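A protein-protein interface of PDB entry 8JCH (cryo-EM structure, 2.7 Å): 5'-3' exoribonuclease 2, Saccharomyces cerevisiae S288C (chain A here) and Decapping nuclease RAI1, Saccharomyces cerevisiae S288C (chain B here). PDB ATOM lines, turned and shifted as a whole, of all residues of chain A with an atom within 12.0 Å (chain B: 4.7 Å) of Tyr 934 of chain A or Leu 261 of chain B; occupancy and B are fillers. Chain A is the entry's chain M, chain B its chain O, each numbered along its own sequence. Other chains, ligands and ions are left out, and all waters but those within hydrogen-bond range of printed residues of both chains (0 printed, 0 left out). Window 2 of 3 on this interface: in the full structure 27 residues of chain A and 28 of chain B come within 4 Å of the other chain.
OH of Tyr 934 of chain A lies within hydrogen-bond range of ND2 of Asn 305 of chain B.
O of Leu 301 of chain B sits close to OD1 of Asn 305 of chain B (3.1 Å).
Among the printed residues, pairs that only touch across the chains: Gly 932 of chain A with Val 248 of chain B (3.7 Å), Gly 933 of chain A with Val 248 of chain B (3.7 Å), Tyr 934 of chain A with Phe 257 of chain B (3.6 Å), Tyr 934 of chain A with Glu 258 of chain B (3.7 Å), Tyr 934 of chain A with Leu 261 of chain B (3.6 Å), Tyr 934 of chain A with Phe 293 of chain B (3.7 Å), Tyr 934 of chain A with Leu 301 of chain B (3.7 Å), Arg 935 of chain A with Phe 293 of chain B (3.2 Å), Phe 937 of chain A with Val 248 of chain B (3.7 Å) and Phe 938 of chain A with Asn 305 of chain B (3.4 Å).
Printed residues of chain B within 4 Å of Gly 932 of chain A: Val 248 (3.7 Å).
Printed residues of chain B within 4 Å of Gly 933 of chain A: Val 248 (3.7 Å).
Of chain B, only Phe 257, Glu 258, Leu 261, Phe 293, Leu 301 and Asn 305 come within 4 Å of Tyr 934 of chain A.
Printed residues of chain B within 4 Å of Arg 935 of chain A: Phe 293.
Printed residues of chain B within 4 Å of Phe 937 of chain A: Val 248.
Of the printed residues of chain B, Phe 938 of chain A touches Asn 305 (3.4 Å).
Val 248 of chain B touches just these residues of chain A: Gly 932 (3.7 Å), Gly 933 (3.7 Å) and Phe 937 (3.7 Å).
Phe 257 of chain B touches just one residue of chain A: Tyr 934.
Of chain A, only Tyr 934 comes within 4 Å of Glu 258 of chain B.
Of chain A, only Tyr 934 comes within 4 Å of Leu 261 of chain B.
No residue of chain A comes within 4 Å of Thr 264 of chain B.
No residue of chain A comes within 4 Å of Val 298 of chain B.
Leu 301 of chain B touches just one residue of chain A: Tyr 934.
No residue of chain A comes within 4 Å of Leu 302 of chain B.
The nearest residue of chain B that does not touch Tyr 934 of chain A is Leu 302 of chain B (4.05 Å).
The nearest residue of chain A that does not touch Leu 261 of chain B is Arg 935 of chain A (7.3 Å).
The nearest printed residue of chain A that does not touch Asn 305 of chain B is Arg 935 of chain A (7.0 Å).
Hydrophobic or aromatic side chains of chain B within 4 Å of the printed part of chain A: Val 248, Phe 257, Leu 261, Phe 293 and Leu 301.
Printed residues of chain A that touch a printed residue of chain B: Gly 932, Gly 933, Tyr 934, Arg 935, Phe 937 and Phe 938.
Hydrophobic or aromatic side chains of chain A that line the printed part of chain B: Tyr 934, Phe 937 and Phe 938.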
ATOM      1  N   THR A 925       3.605  23.849   1.101  1.00  0.00           N
ATOM      2  CA  THR A 925       4.737  22.947   1.262  1.00  0.00           C
ATOM      3  C   THR A 925       4.267  21.498   1.246  1.00  0.00           C
ATOM      4  O   THR A 925       3.273  21.148   1.890  1.00  0.00           O
ATOM      5  CB  THR A 925       5.474  23.249   2.567  1.00  0.00           C
ATOM      6  OG1 THR A 925       5.681  24.662   2.686  1.00  0.00           O
ATOM      7  CG2 THR A 925       6.821  22.541   2.598  1.00  0.00           C
ATOM      8  N   LYS A 928       6.203  17.783   5.546  1.00  0.00           N
ATOM      9  CA  LYS A 928       5.866  18.132   6.914  1.00  0.00           C
ATOM     10  C   LYS A 928       7.124  18.564   7.669  1.00  0.00           C
ATOM     11  O   LYS A 928       8.238  18.171   7.309  1.00  0.00           O
ATOM     12  CB  LYS A 928       5.206  16.949   7.621  1.00  0.00           C
ATOM     13  CG  LYS A 928       6.145  15.802   7.947  1.00  0.00           C
ATOM     14  CD  LYS A 928       5.568  14.914   9.037  1.00  0.00           C
ATOM     15  CE  LYS A 928       6.579  13.878   9.502  1.00  0.00           C
ATOM     16  NZ  LYS A 928       6.109  12.489   9.245  1.00  0.00           N
ATOM     17  N   PRO A 929       6.977  19.391   8.704  1.00  0.00           N
ATOM     18  CA  PRO A 929       8.156  19.852   9.449  1.00  0.00           C
ATOM     19  C   PRO A 929       8.899  18.692  10.097  1.00  0.00           C
ATOM     20  O   PRO A 929       8.317  17.882  10.822  1.00  0.00           O
ATOM     21  CB  PRO A 929       7.567  20.805  10.497  1.00  0.00           C
ATOM     22  CG  PRO A 929       6.116  20.453  10.575  1.00  0.00           C
ATOM     23  CD  PRO A 929       5.737  20.012   9.199  1.00  0.00           C
ATOM     24  N   ARG A 930      10.199  18.620   9.825  1.00  0.00           N
ATOM     25  CA  ARG A 930      11.092  17.594  10.357  1.00  0.00           C
ATOM     26  C   ARG A 930      12.350  18.242  10.920  1.00  0.00           C
ATOM     27  O   ARG A 930      13.477  17.849  10.609  1.00  0.00           O
ATOM     28  CB  ARG A 930      11.442  16.563   9.288  1.00  0.00           C
ATOM     29  CG  ARG A 930      11.296  17.070   7.863  1.00  0.00           C
ATOM     30  CD  ARG A 930      11.546  15.960   6.856  1.00  0.00           C
ATOM     31  NE  ARG A 930      10.617  14.848   7.020  1.00  0.00           N
ATOM     32  CZ  ARG A 930       9.362  14.850   6.591  1.00  0.00           C
ATOM     33  NH1 ARG A 930       8.848  15.893   5.959  1.00  0.00           N
ATOM     34  NH2 ARG A 930       8.605  13.776   6.798  1.00  0.00           N
ATOM     35  N   THR A 931      12.154  19.268  11.752  1.00  0.00           N
ATOM     36  CA  THR A 931      13.230  20.079  12.316  1.00  0.00           C
ATOM     37  C   THR A 931      14.041  20.746  11.211  1.00  0.00           C
ATOM     38  O   THR A 931      13.562  20.887  10.081  1.00  0.00           O
ATOM     39  CB  THR A 931      14.145  19.249  13.225  1.00  0.00           C
ATOM     40  OG1 THR A 931      14.954  18.373  12.428  1.00  0.00           O
ATOM     41  CG2 THR A 931      13.324  18.425  14.208  1.00  0.00           C
ATOM     42  N   GLY A 932      15.265  21.159  11.526  1.00  0.00           N
ATOM     43  CA  GLY A 932      16.076  21.888  10.571  1.00  0.00           C
ATOM     44  C   GLY A 932      16.397  23.295  11.032  1.00  0.00           C
ATOM     45  O   GLY A 932      17.161  23.481  11.984  1.00  0.00           O
ATOM     46  N   GLY A 933      15.823  24.293  10.369  1.00  0.00           N
ATOM     47  CA  GLY A 933      16.080  25.668  10.749  1.00  0.00           C
ATOM     48  C   GLY A 933      15.118  26.611  10.062  1.00  0.00           C
ATOM     49  O   GLY A 933      14.261  26.199   9.275  1.00  0.00           O
ATOM     50  N   TYR A 934      15.276  27.897  10.384  1.00  0.00           N
ATOM     51  CA  TYR A 934      14.466  28.973   9.823  1.00  0.00           C
ATOM     52  C   TYR A 934      12.982  28.752  10.087  1.00  0.00           C
ATOM     53  O   TYR A 934      12.489  29.047  11.182  1.00  0.00           O
ATOM     54  CB  TYR A 934      14.723  29.112   8.320  1.00  0.00           C
ATOM     55  CG  TYR A 934      14.409  30.484   7.770  1.00  0.00           C
ATOM     56  CD1 TYR A 934      15.303  31.535   7.922  1.00  0.00           C
ATOM     57  CD2 TYR A 934      13.219  30.729   7.098  1.00  0.00           C
ATOM     58  CE1 TYR A 934      15.021  32.792   7.421  1.00  0.00           C
ATOM     59  CE2 TYR A 934      12.927  31.983   6.594  1.00  0.00           C
ATOM     60  CZ  TYR A 934      13.832  33.010   6.758  1.00  0.00           C
ATOM     61  OH  TYR A 934      13.547  34.259   6.257  1.00  0.00           O
ATOM     62  N   ARG A 935      12.260  28.243   9.085  1.00  0.00           N
ATOM     63  CA  ARG A 935      10.831  28.003   9.252  1.00  0.00           C
ATOM     64  C   ARG A 935      10.569  26.937  10.309  1.00  0.00           C
ATOM     65  O   ARG A 935       9.626  27.057  11.099  1.00  0.00           O
ATOM     66  CB  ARG A 935      10.202  27.604   7.917  1.00  0.00           C
ATOM     67  CG  ARG A 935      11.044  26.651   7.085  1.00  0.00           C
ATOM     68  CD  ARG A 935      10.229  26.025   5.961  1.00  0.00           C
ATOM     69  NE  ARG A 935       9.775  27.012   4.987  1.00  0.00           N
ATOM     70  CZ  ARG A 935       8.545  27.506   4.937  1.00  0.00           C
ATOM     71  NH1 ARG A 935       7.613  27.126   5.794  1.00  0.00           N
ATOM     72  NH2 ARG A 935       8.243  28.403   4.002  1.00  0.00           N
ATOM     73  N   ALA A 936      11.392  25.887  10.338  1.00  0.00           N
ATOM     74  CA  ALA A 936      11.238  24.857  11.361  1.00  0.00           C
ATOM     75  C   ALA A 936      11.474  25.424  12.754  1.00  0.00           C
ATOM     76  O   ALA A 936      10.738  25.104  13.697  1.00  0.00           O
ATOM     77  CB  ALA A 936      12.190  23.696  11.084  1.00  0.00           C
ATOM     78  N   PHE A 937      12.499  26.267  12.906  1.00  0.00           N
ATOM     79  CA  PHE A 937      12.759  26.891  14.200  1.00  0.00           C
ATOM     80  C   PHE A 937      11.607  27.798  14.616  1.00  0.00           C
ATOM     81  O   PHE A 937      11.211  27.812  15.787  1.00  0.00           O
ATOM     82  CB  PHE A 937      14.070  27.675  14.151  1.00  0.00           C
ATOM     83  CG  PHE A 937      14.959  27.441  15.338  1.00  0.00           C
ATOM     84  CD1 PHE A 937      14.429  27.376  16.616  1.00  0.00           C
ATOM     85  CD2 PHE A 937      16.327  27.288  15.177  1.00  0.00           C
ATOM     86  CE1 PHE A 937      15.246  27.162  17.711  1.00  0.00           C
ATOM     87  CE2 PHE A 937      17.148  27.073  16.268  1.00  0.00           C
ATOM     88  CZ  PHE A 937      16.607  27.011  17.536  1.00  0.00           C
ATOM     89  N   PHE A 938      11.059  28.564  13.670  1.00  0.00           N
ATOM     90  CA  PHE A 938       9.922  29.425  13.982  1.00  0.00           C
ATOM     91  C   PHE A 938       8.707  28.605  14.399  1.00  0.00           C
ATOM     92  O   PHE A 938       7.999  28.966  15.347  1.00  0.00           O
ATOM     93  CB  PHE A 938       9.587  30.311  12.783  1.00  0.00           C
ATOM     94  CG  PHE A 938      10.646  31.328  12.465  1.00  0.00           C
ATOM     95  CD1 PHE A 938      11.494  31.798  13.454  1.00  0.00           C
ATOM     96  CD2 PHE A 938      10.792  31.816  11.177  1.00  0.00           C
ATOM     97  CE1 PHE A 938      12.469  32.735  13.164  1.00  0.00           C
ATOM     98  CE2 PHE A 938      11.764  32.753  10.881  1.00  0.00           C
ATOM     99  CZ  PHE A 938      12.603  33.213  11.876  1.00  0.00           C
ATOM    100  N   TYR A 939       8.451  27.496  13.702  1.00  0.00           N
ATOM    101  CA  TYR A 939       7.333  26.629  14.064  1.00  0.00           C
ATOM    102  C   TYR A 939       7.529  26.029  15.449  1.00  0.00           C
ATOM    103  O   TYR A 939       6.583  25.954  16.242  1.00  0.00           O
ATOM    104  CB  TYR A 939       7.166  25.530  13.013  1.00  0.00           C
ATOM    105  CG  TYR A 939       6.155  24.464  13.378  1.00  0.00           C
ATOM    106  CD1 TYR A 939       4.805  24.638  13.103  1.00  0.00           C
ATOM    107  CD2 TYR A 939       6.553  23.276  13.980  1.00  0.00           C
ATOM    108  CE1 TYR A 939       3.878  23.666  13.429  1.00  0.00           C
ATOM    109  CE2 TYR A 939       5.632  22.299  14.310  1.00  0.00           C
ATOM    110  CZ  TYR A 939       4.297  22.499  14.032  1.00  0.00           C
ATOM    111  OH  TYR A 939       3.378  21.528  14.358  1.00  0.00           O
ATOM    112  N   PHE A 940       8.752  25.591  15.760  1.00  0.00           N
ATOM    113  CA  PHE A 940       9.029  25.043  17.084  1.00  0.00           C
ATOM    114  C   PHE A 940       8.842  26.097  18.168  1.00  0.00           C
ATOM    115  O   PHE A 940       8.288  25.810  19.236  1.00  0.00           O
ATOM    116  CB  PHE A 940      10.445  24.469  17.130  1.00  0.00           C
ATOM    117  CG  PHE A 940      10.534  23.038  16.677  1.00  0.00           C
ATOM    118  CD1 PHE A 940       9.507  22.460  15.949  1.00  0.00           C
ATOM    119  CD2 PHE A 940      11.648  22.271  16.980  1.00  0.00           C
ATOM    120  CE1 PHE A 940       9.587  21.145  15.532  1.00  0.00           C
ATOM    121  CE2 PHE A 940      11.734  20.955  16.566  1.00  0.00           C
ATOM    122  CZ  PHE A 940      10.703  20.392  15.841  1.00  0.00           C
ATOM    123  N   ALA A 941       9.299  27.326  17.912  1.00  0.00           N
ATOM    124  CA  ALA A 941       9.123  28.401  18.884  1.00  0.00           C
ATOM    125  C   ALA A 941       7.647  28.720  19.092  1.00  0.00           C
ATOM    126  O   ALA A 941       7.210  28.959  20.225  1.00  0.00           O
ATOM    127  CB  ALA A 941       9.884  29.647  18.433  1.00  0.00           C
ATOM    128  N   GLU A 942       6.866  28.736  18.009  1.00  0.00           N
ATOM    129  CA  GLU A 942       5.433  28.979  18.134  1.00  0.00           C
ATOM    130  C   GLU A 942       4.750  27.865  18.918  1.00  0.00           C
ATOM    131  O   GLU A 942       3.863  28.127  19.739  1.00  0.00           O
ATOM    132  CB  GLU A 942       4.802  29.125  16.749  1.00  0.00           C
ATOM    133  CG  GLU A 942       3.385  29.676  16.766  1.00  0.00           C
ATOM    134  CD  GLU A 942       3.332  31.160  16.461  1.00  0.00           C
ATOM    135  OE1 GLU A 942       3.274  31.521  15.267  1.00  0.00           O
ATOM    136  OE2 GLU A 942       3.348  31.965  17.416  1.00  0.00           O
ATOM    137  N   LEU A 943       5.146  26.614  18.671  1.00  0.00           N
ATOM    138  CA  LEU A 943       4.570  25.494  19.411  1.00  0.00           C
ATOM    139  C   LEU A 943       4.920  25.579  20.892  1.00  0.00           C
ATOM    140  O   LEU A 943       4.071  25.325  21.754  1.00  0.00           O
ATOM    141  CB  LEU A 943       5.049  24.171  18.806  1.00  0.00           C
ATOM    142  CG  LEU A 943       4.590  22.821  19.375  1.00  0.00           C
ATOM    143  CD1 LEU A 943       5.479  22.339  20.521  1.00  0.00           C
ATOM    144  CD2 LEU A 943       3.126  22.868  19.803  1.00  0.00           C
ATOM    145  N   VAL B 248      21.190  24.788  11.484  1.00  0.00           N
ATOM    146  CA  VAL B 248      21.429  25.899  12.397  1.00  0.00           C
ATOM    147  C   VAL B 248      21.416  25.400  13.839  1.00  0.00           C
ATOM    148  O   VAL B 248      20.812  24.376  14.172  1.00  0.00           O
ATOM    149  CB  VAL B 248      20.397  27.022  12.185  1.00  0.00           C
ATOM    150  CG1 VAL B 248      20.330  27.409  10.715  1.00  0.00           C
ATOM    151  CG2 VAL B 248      19.030  26.595  12.695  1.00  0.00           C
ATOM    152  N   PHE B 257      22.050  31.793   7.402  1.00  0.00           N
ATOM    153  CA  PHE B 257      21.029  31.277   6.498  1.00  0.00           C
ATOM    154  C   PHE B 257      20.190  32.405   5.913  1.00  0.00           C
ATOM    155  O   PHE B 257      19.771  32.336   4.754  1.00  0.00           O
ATOM    156  CB  PHE B 257      20.140  30.268   7.225  1.00  0.00           C
ATOM    157  CG  PHE B 257      19.256  29.473   6.307  1.00  0.00           C
ATOM    158  CD1 PHE B 257      19.788  28.818   5.209  1.00  0.00           C
ATOM    159  CD2 PHE B 257      17.894  29.384   6.539  1.00  0.00           C
ATOM    160  CE1 PHE B 257      18.978  28.087   4.361  1.00  0.00           C
ATOM    161  CE2 PHE B 257      17.079  28.654   5.694  1.00  0.00           C
ATOM    162  CZ  PHE B 257      17.622  28.005   4.604  1.00  0.00           C
ATOM    163  N   GLU B 258      19.931  33.451   6.702  1.00  0.00           N
ATOM    164  CA  GLU B 258      19.217  34.612   6.179  1.00  0.00           C
ATOM    165  C   GLU B 258      20.017  35.300   5.081  1.00  0.00           C
ATOM    166  O   GLU B 258      19.453  35.738   4.073  1.00  0.00           O
ATOM    167  CB  GLU B 258      18.905  35.590   7.313  1.00  0.00           C
ATOM    168  CG  GLU B 258      17.714  35.188   8.167  1.00  0.00           C
ATOM    169  CD  GLU B 258      17.791  35.748   9.574  1.00  0.00           C
ATOM    170  OE1 GLU B 258      18.594  36.676   9.803  1.00  0.00           O
ATOM    171  OE2 GLU B 258      17.048  35.259  10.451  1.00  0.00           O
ATOM    172  N   ARG B 259      21.334  35.411   5.262  1.00  0.00           N
ATOM    173  CA  ARG B 259      22.181  35.989   4.220  1.00  0.00           C
ATOM    174  C   ARG B 259      22.186  35.119   2.967  1.00  0.00           C
ATOM    175  O   ARG B 259      22.164  35.633   1.840  1.00  0.00           O
ATOM    176  CB  ARG B 259      23.601  36.184   4.748  1.00  0.00           C
ATOM    177  CG  ARG B 259      23.796  37.469   5.536  1.00  0.00           C
ATOM    178  CD  ARG B 259      24.967  37.358   6.499  1.00  0.00           C
ATOM    179  NE  ARG B 259      25.209  38.609   7.207  1.00  0.00           N
ATOM    180  CZ  ARG B 259      24.548  38.998   8.290  1.00  0.00           C
ATOM    181  NH1 ARG B 259      23.591  38.254   8.821  1.00  0.00           N
ATOM    182  NH2 ARG B 259      24.854  40.163   8.854  1.00  0.00           N
ATOM    183  N   LYS B 260      22.226  33.796   3.142  1.00  0.00           N
ATOM    184  CA  LYS B 260      22.157  32.899   1.991  1.00  0.00           C
ATOM    185  C   LYS B 260      20.823  33.040   1.264  1.00  0.00           C
ATOM    186  O   LYS B 260      20.772  33.007   0.027  1.00  0.00           O
ATOM    187  CB  LYS B 260      22.379  31.454   2.437  1.00  0.00           C
ATOM    188  CG  LYS B 260      23.779  31.176   2.960  1.00  0.00           C
ATOM    189  CD  LYS B 260      24.839  31.600   1.957  1.00  0.00           C
ATOM    190  CE  LYS B 260      25.044  30.542   0.886  1.00  0.00           C
ATOM    191  NZ  LYS B 260      25.618  29.288   1.448  1.00  0.00           N
ATOM    192  N   LEU B 261      19.732  33.186   2.018  1.00  0.00           N
ATOM    193  CA  LEU B 261      18.425  33.411   1.407  1.00  0.00           C
ATOM    194  C   LEU B 261      18.381  34.748   0.679  1.00  0.00           C
ATOM    195  O   LEU B 261      17.758  34.861  -0.380  1.00  0.00           O
ATOM    196  CB  LEU B 261      17.329  33.337   2.469  1.00  0.00           C
ATOM    197  CG  LEU B 261      17.019  31.943   3.016  1.00  0.00           C
ATOM    198  CD1 LEU B 261      15.847  31.992   3.982  1.00  0.00           C
ATOM    199  CD2 LEU B 261      16.744  30.968   1.880  1.00  0.00           C
ATOM    200  N   PHE B 262      19.027  35.773   1.238  1.00  0.00           N
ATOM    201  CA  PHE B 262      19.175  37.046   0.538  1.00  0.00           C
ATOM    202  C   PHE B 262      19.873  36.845  -0.803  1.00  0.00           C
ATOM    203  O   PHE B 262      19.412  37.339  -1.841  1.00  0.00           O
ATOM    204  CB  PHE B 262      19.955  38.023   1.425  1.00  0.00           C
ATOM    205  CG  PHE B 262      20.157  39.398   0.829  1.00  0.00           C
ATOM    206  CD1 PHE B 262      19.391  39.853  -0.232  1.00  0.00           C
ATOM    207  CD2 PHE B 262      21.134  40.236   1.343  1.00  0.00           C
ATOM    208  CE1 PHE B 262      19.597  41.111  -0.769  1.00  0.00           C
ATOM    209  CE2 PHE B 262      21.341  41.495   0.814  1.00  0.00           C
ATOM    210  CZ  PHE B 262      20.571  41.934  -0.242  1.00  0.00           C
ATOM    211  N   ARG B 263      20.988  36.114  -0.796  1.00  0.00           N
ATOM    212  CA  ARG B 263      21.735  35.896  -2.032  1.00  0.00           C
ATOM    213  C   ARG B 263      20.901  35.138  -3.058  1.00  0.00           C
ATOM    214  O   ARG B 263      20.860  35.513  -4.239  1.00  0.00           O
ATOM    215  CB  ARG B 263      23.034  35.147  -1.732  1.00  0.00           C
ATOM    216  CG  ARG B 263      24.035  35.957  -0.927  1.00  0.00           C
ATOM    217  CD  ARG B 263      25.364  35.231  -0.790  1.00  0.00           C
ATOM    218  NE  ARG B 263      26.312  35.991   0.015  1.00  0.00           N
ATOM    219  CZ  ARG B 263      27.536  35.582   0.318  1.00  0.00           C
ATOM    220  NH1 ARG B 263      27.999  34.416  -0.101  1.00  0.00           N
ATOM    221  NH2 ARG B 263      28.314  36.363   1.063  1.00  0.00           N
ATOM    222  N   THR B 264      20.206  34.081  -2.628  1.00  0.00           N
ATOM    223  CA  THR B 264      19.419  33.298  -3.576  1.00  0.00           C
ATOM    224  C   THR B 264      18.186  34.059  -4.055  1.00  0.00           C
ATOM    225  O   THR B 264      17.756  33.876  -5.200  1.00  0.00           O
ATOM    226  CB  THR B 264      19.031  31.946  -2.966  1.00  0.00           C
ATOM    227  OG1 THR B 264      18.608  31.056  -4.006  1.00  0.00           O
ATOM    228  CG2 THR B 264      17.913  32.092  -1.946  1.00  0.00           C
ATOM    229  N   TRP B 265      17.619  34.934  -3.219  1.00  0.00           N
ATOM    230  CA  TRP B 265      16.494  35.750  -3.659  1.00  0.00           C
ATOM    231  C   TRP B 265      16.942  36.798  -4.666  1.00  0.00           C
ATOM    232  O   TRP B 265      16.225  37.082  -5.631  1.00  0.00           O
ATOM    233  CB  TRP B 265      15.818  36.414  -2.459  1.00  0.00           C
ATOM    234  CG  TRP B 265      14.719  37.355  -2.847  1.00  0.00           C
ATOM    235  CD1 TRP B 265      13.415  37.037  -3.093  1.00  0.00           C
ATOM    236  CD2 TRP B 265      14.831  38.770  -3.041  1.00  0.00           C
ATOM    237  NE1 TRP B 265      12.708  38.167  -3.424  1.00  0.00           N
ATOM    238  CE2 TRP B 265      13.554  39.244  -3.400  1.00  0.00           C
ATOM    239  CE3 TRP B 265      15.886  39.681  -2.945  1.00  0.00           C
ATOM    240  CZ2 TRP B 265      13.304  40.589  -3.662  1.00  0.00           C
ATOM    241  CZ3 TRP B 265      15.637  41.016  -3.205  1.00  0.00           C
ATOM    242  CH2 TRP B 265      14.356  41.458  -3.559  1.00  0.00           C
ATOM    243  N   TYR B 278      15.644  24.354  -0.884  1.00  0.00           N
ATOM    244  CA  TYR B 278      16.931  24.287  -0.209  1.00  0.00           C
ATOM    245  C   TYR B 278      17.032  22.990   0.582  1.00  0.00           C
ATOM    246  O   TYR B 278      16.029  22.464   1.073  1.00  0.00           O
ATOM    247  CB  TYR B 278      17.128  25.484   0.732  1.00  0.00           C
ATOM    248  CG  TYR B 278      18.485  26.144   0.640  1.00  0.00           C
ATOM    249  CD1 TYR B 278      19.649  25.391   0.655  1.00  0.00           C
ATOM    250  CD2 TYR B 278      18.598  27.525   0.542  1.00  0.00           C
ATOM    251  CE1 TYR B 278      20.890  25.993   0.576  1.00  0.00           C
ATOM    252  CE2 TYR B 278      19.835  28.137   0.460  1.00  0.00           C
ATOM    253  CZ  TYR B 278      20.977  27.366   0.477  1.00  0.00           C
ATOM    254  OH  TYR B 278      22.212  27.969   0.396  1.00  0.00           O
ATOM    255  N   PHE B 293      10.310  26.929  -0.603  1.00  0.00           N
ATOM    256  CA  PHE B 293      10.189  28.382  -0.685  1.00  0.00           C
ATOM    257  C   PHE B 293       9.656  28.815  -2.047  1.00  0.00           C
ATOM    258  O   PHE B 293       9.942  28.202  -3.078  1.00  0.00           O
ATOM    259  CB  PHE B 293      11.541  29.054  -0.434  1.00  0.00           C
ATOM    260  CG  PHE B 293      11.878  29.226   1.018  1.00  0.00           C
ATOM    261  CD1 PHE B 293      10.879  29.353   1.968  1.00  0.00           C
ATOM    262  CD2 PHE B 293      13.199  29.265   1.435  1.00  0.00           C
ATOM    263  CE1 PHE B 293      11.190  29.512   3.306  1.00  0.00           C
ATOM    264  CE2 PHE B 293      13.516  29.423   2.769  1.00  0.00           C
ATOM    265  CZ  PHE B 293      12.511  29.547   3.707  1.00  0.00           C
ATOM    266  N   VAL B 298       9.384  34.607  -0.207  1.00  0.00           N
ATOM    267  CA  VAL B 298      10.691  34.817   0.422  1.00  0.00           C
ATOM    268  C   VAL B 298      10.903  36.261   0.870  1.00  0.00           C
ATOM    269  O   VAL B 298      11.296  36.471   2.030  1.00  0.00           O
ATOM    270  CB  VAL B 298      11.810  34.314  -0.507  1.00  0.00           C
ATOM    271  CG1 VAL B 298      13.136  34.976  -0.157  1.00  0.00           C
ATOM    272  CG2 VAL B 298      11.928  32.800  -0.423  1.00  0.00           C
ATOM    273  N   LEU B 301       8.735  37.189   4.210  1.00  0.00           N
ATOM    274  CA  LEU B 301       9.264  36.610   5.441  1.00  0.00           C
ATOM    275  C   LEU B 301      10.633  37.188   5.776  1.00  0.00           C
ATOM    276  O   LEU B 301      10.956  37.397   6.952  1.00  0.00           O
ATOM    277  CB  LEU B 301       9.338  35.088   5.315  1.00  0.00           C
ATOM    278  CG  LEU B 301       9.564  34.305   6.610  1.00  0.00           C
ATOM    279  CD1 LEU B 301       8.683  34.843   7.730  1.00  0.00           C
ATOM    280  CD2 LEU B 301       9.312  32.820   6.391  1.00  0.00           C
ATOM    281  N   LEU B 302      11.452  37.448   4.753  1.00  0.00           N
ATOM    282  CA  LEU B 302      12.774  38.020   4.979  1.00  0.00           C
ATOM    283  C   LEU B 302      12.674  39.402   5.616  1.00  0.00           C
ATOM    284  O   LEU B 302      13.434  39.726   6.537  1.00  0.00           O
ATOM    285  CB  LEU B 302      13.535  38.078   3.653  1.00  0.00           C
ATOM    286  CG  LEU B 302      15.037  38.366   3.639  1.00  0.00           C
ATOM    287  CD1 LEU B 302      15.297  39.858   3.507  1.00  0.00           C
ATOM    288  CD2 LEU B 302      15.714  37.796   4.877  1.00  0.00           C
ATOM    289  N   ASN B 305      11.335  39.049   9.318  1.00  0.00           N
ATOM    290  CA  ASN B 305      12.336  38.607  10.284  1.00  0.00           C
ATOM    291  C   ASN B 305      13.187  39.777  10.766  1.00  0.00           C
ATOM    292  O   ASN B 305      13.215  40.092  11.961  1.00  0.00           O
ATOM    293  CB  ASN B 305      13.211  37.515   9.666  1.00  0.00           C
ATOM    294  CG  ASN B 305      12.459  36.215   9.460  1.00  0.00           C
ATOM    295  OD1 ASN B 305      11.266  36.121   9.747  1.00  0.00           O
ATOM    296  ND2 ASN B 305      13.157  35.201   8.960  1.00  0.00           N
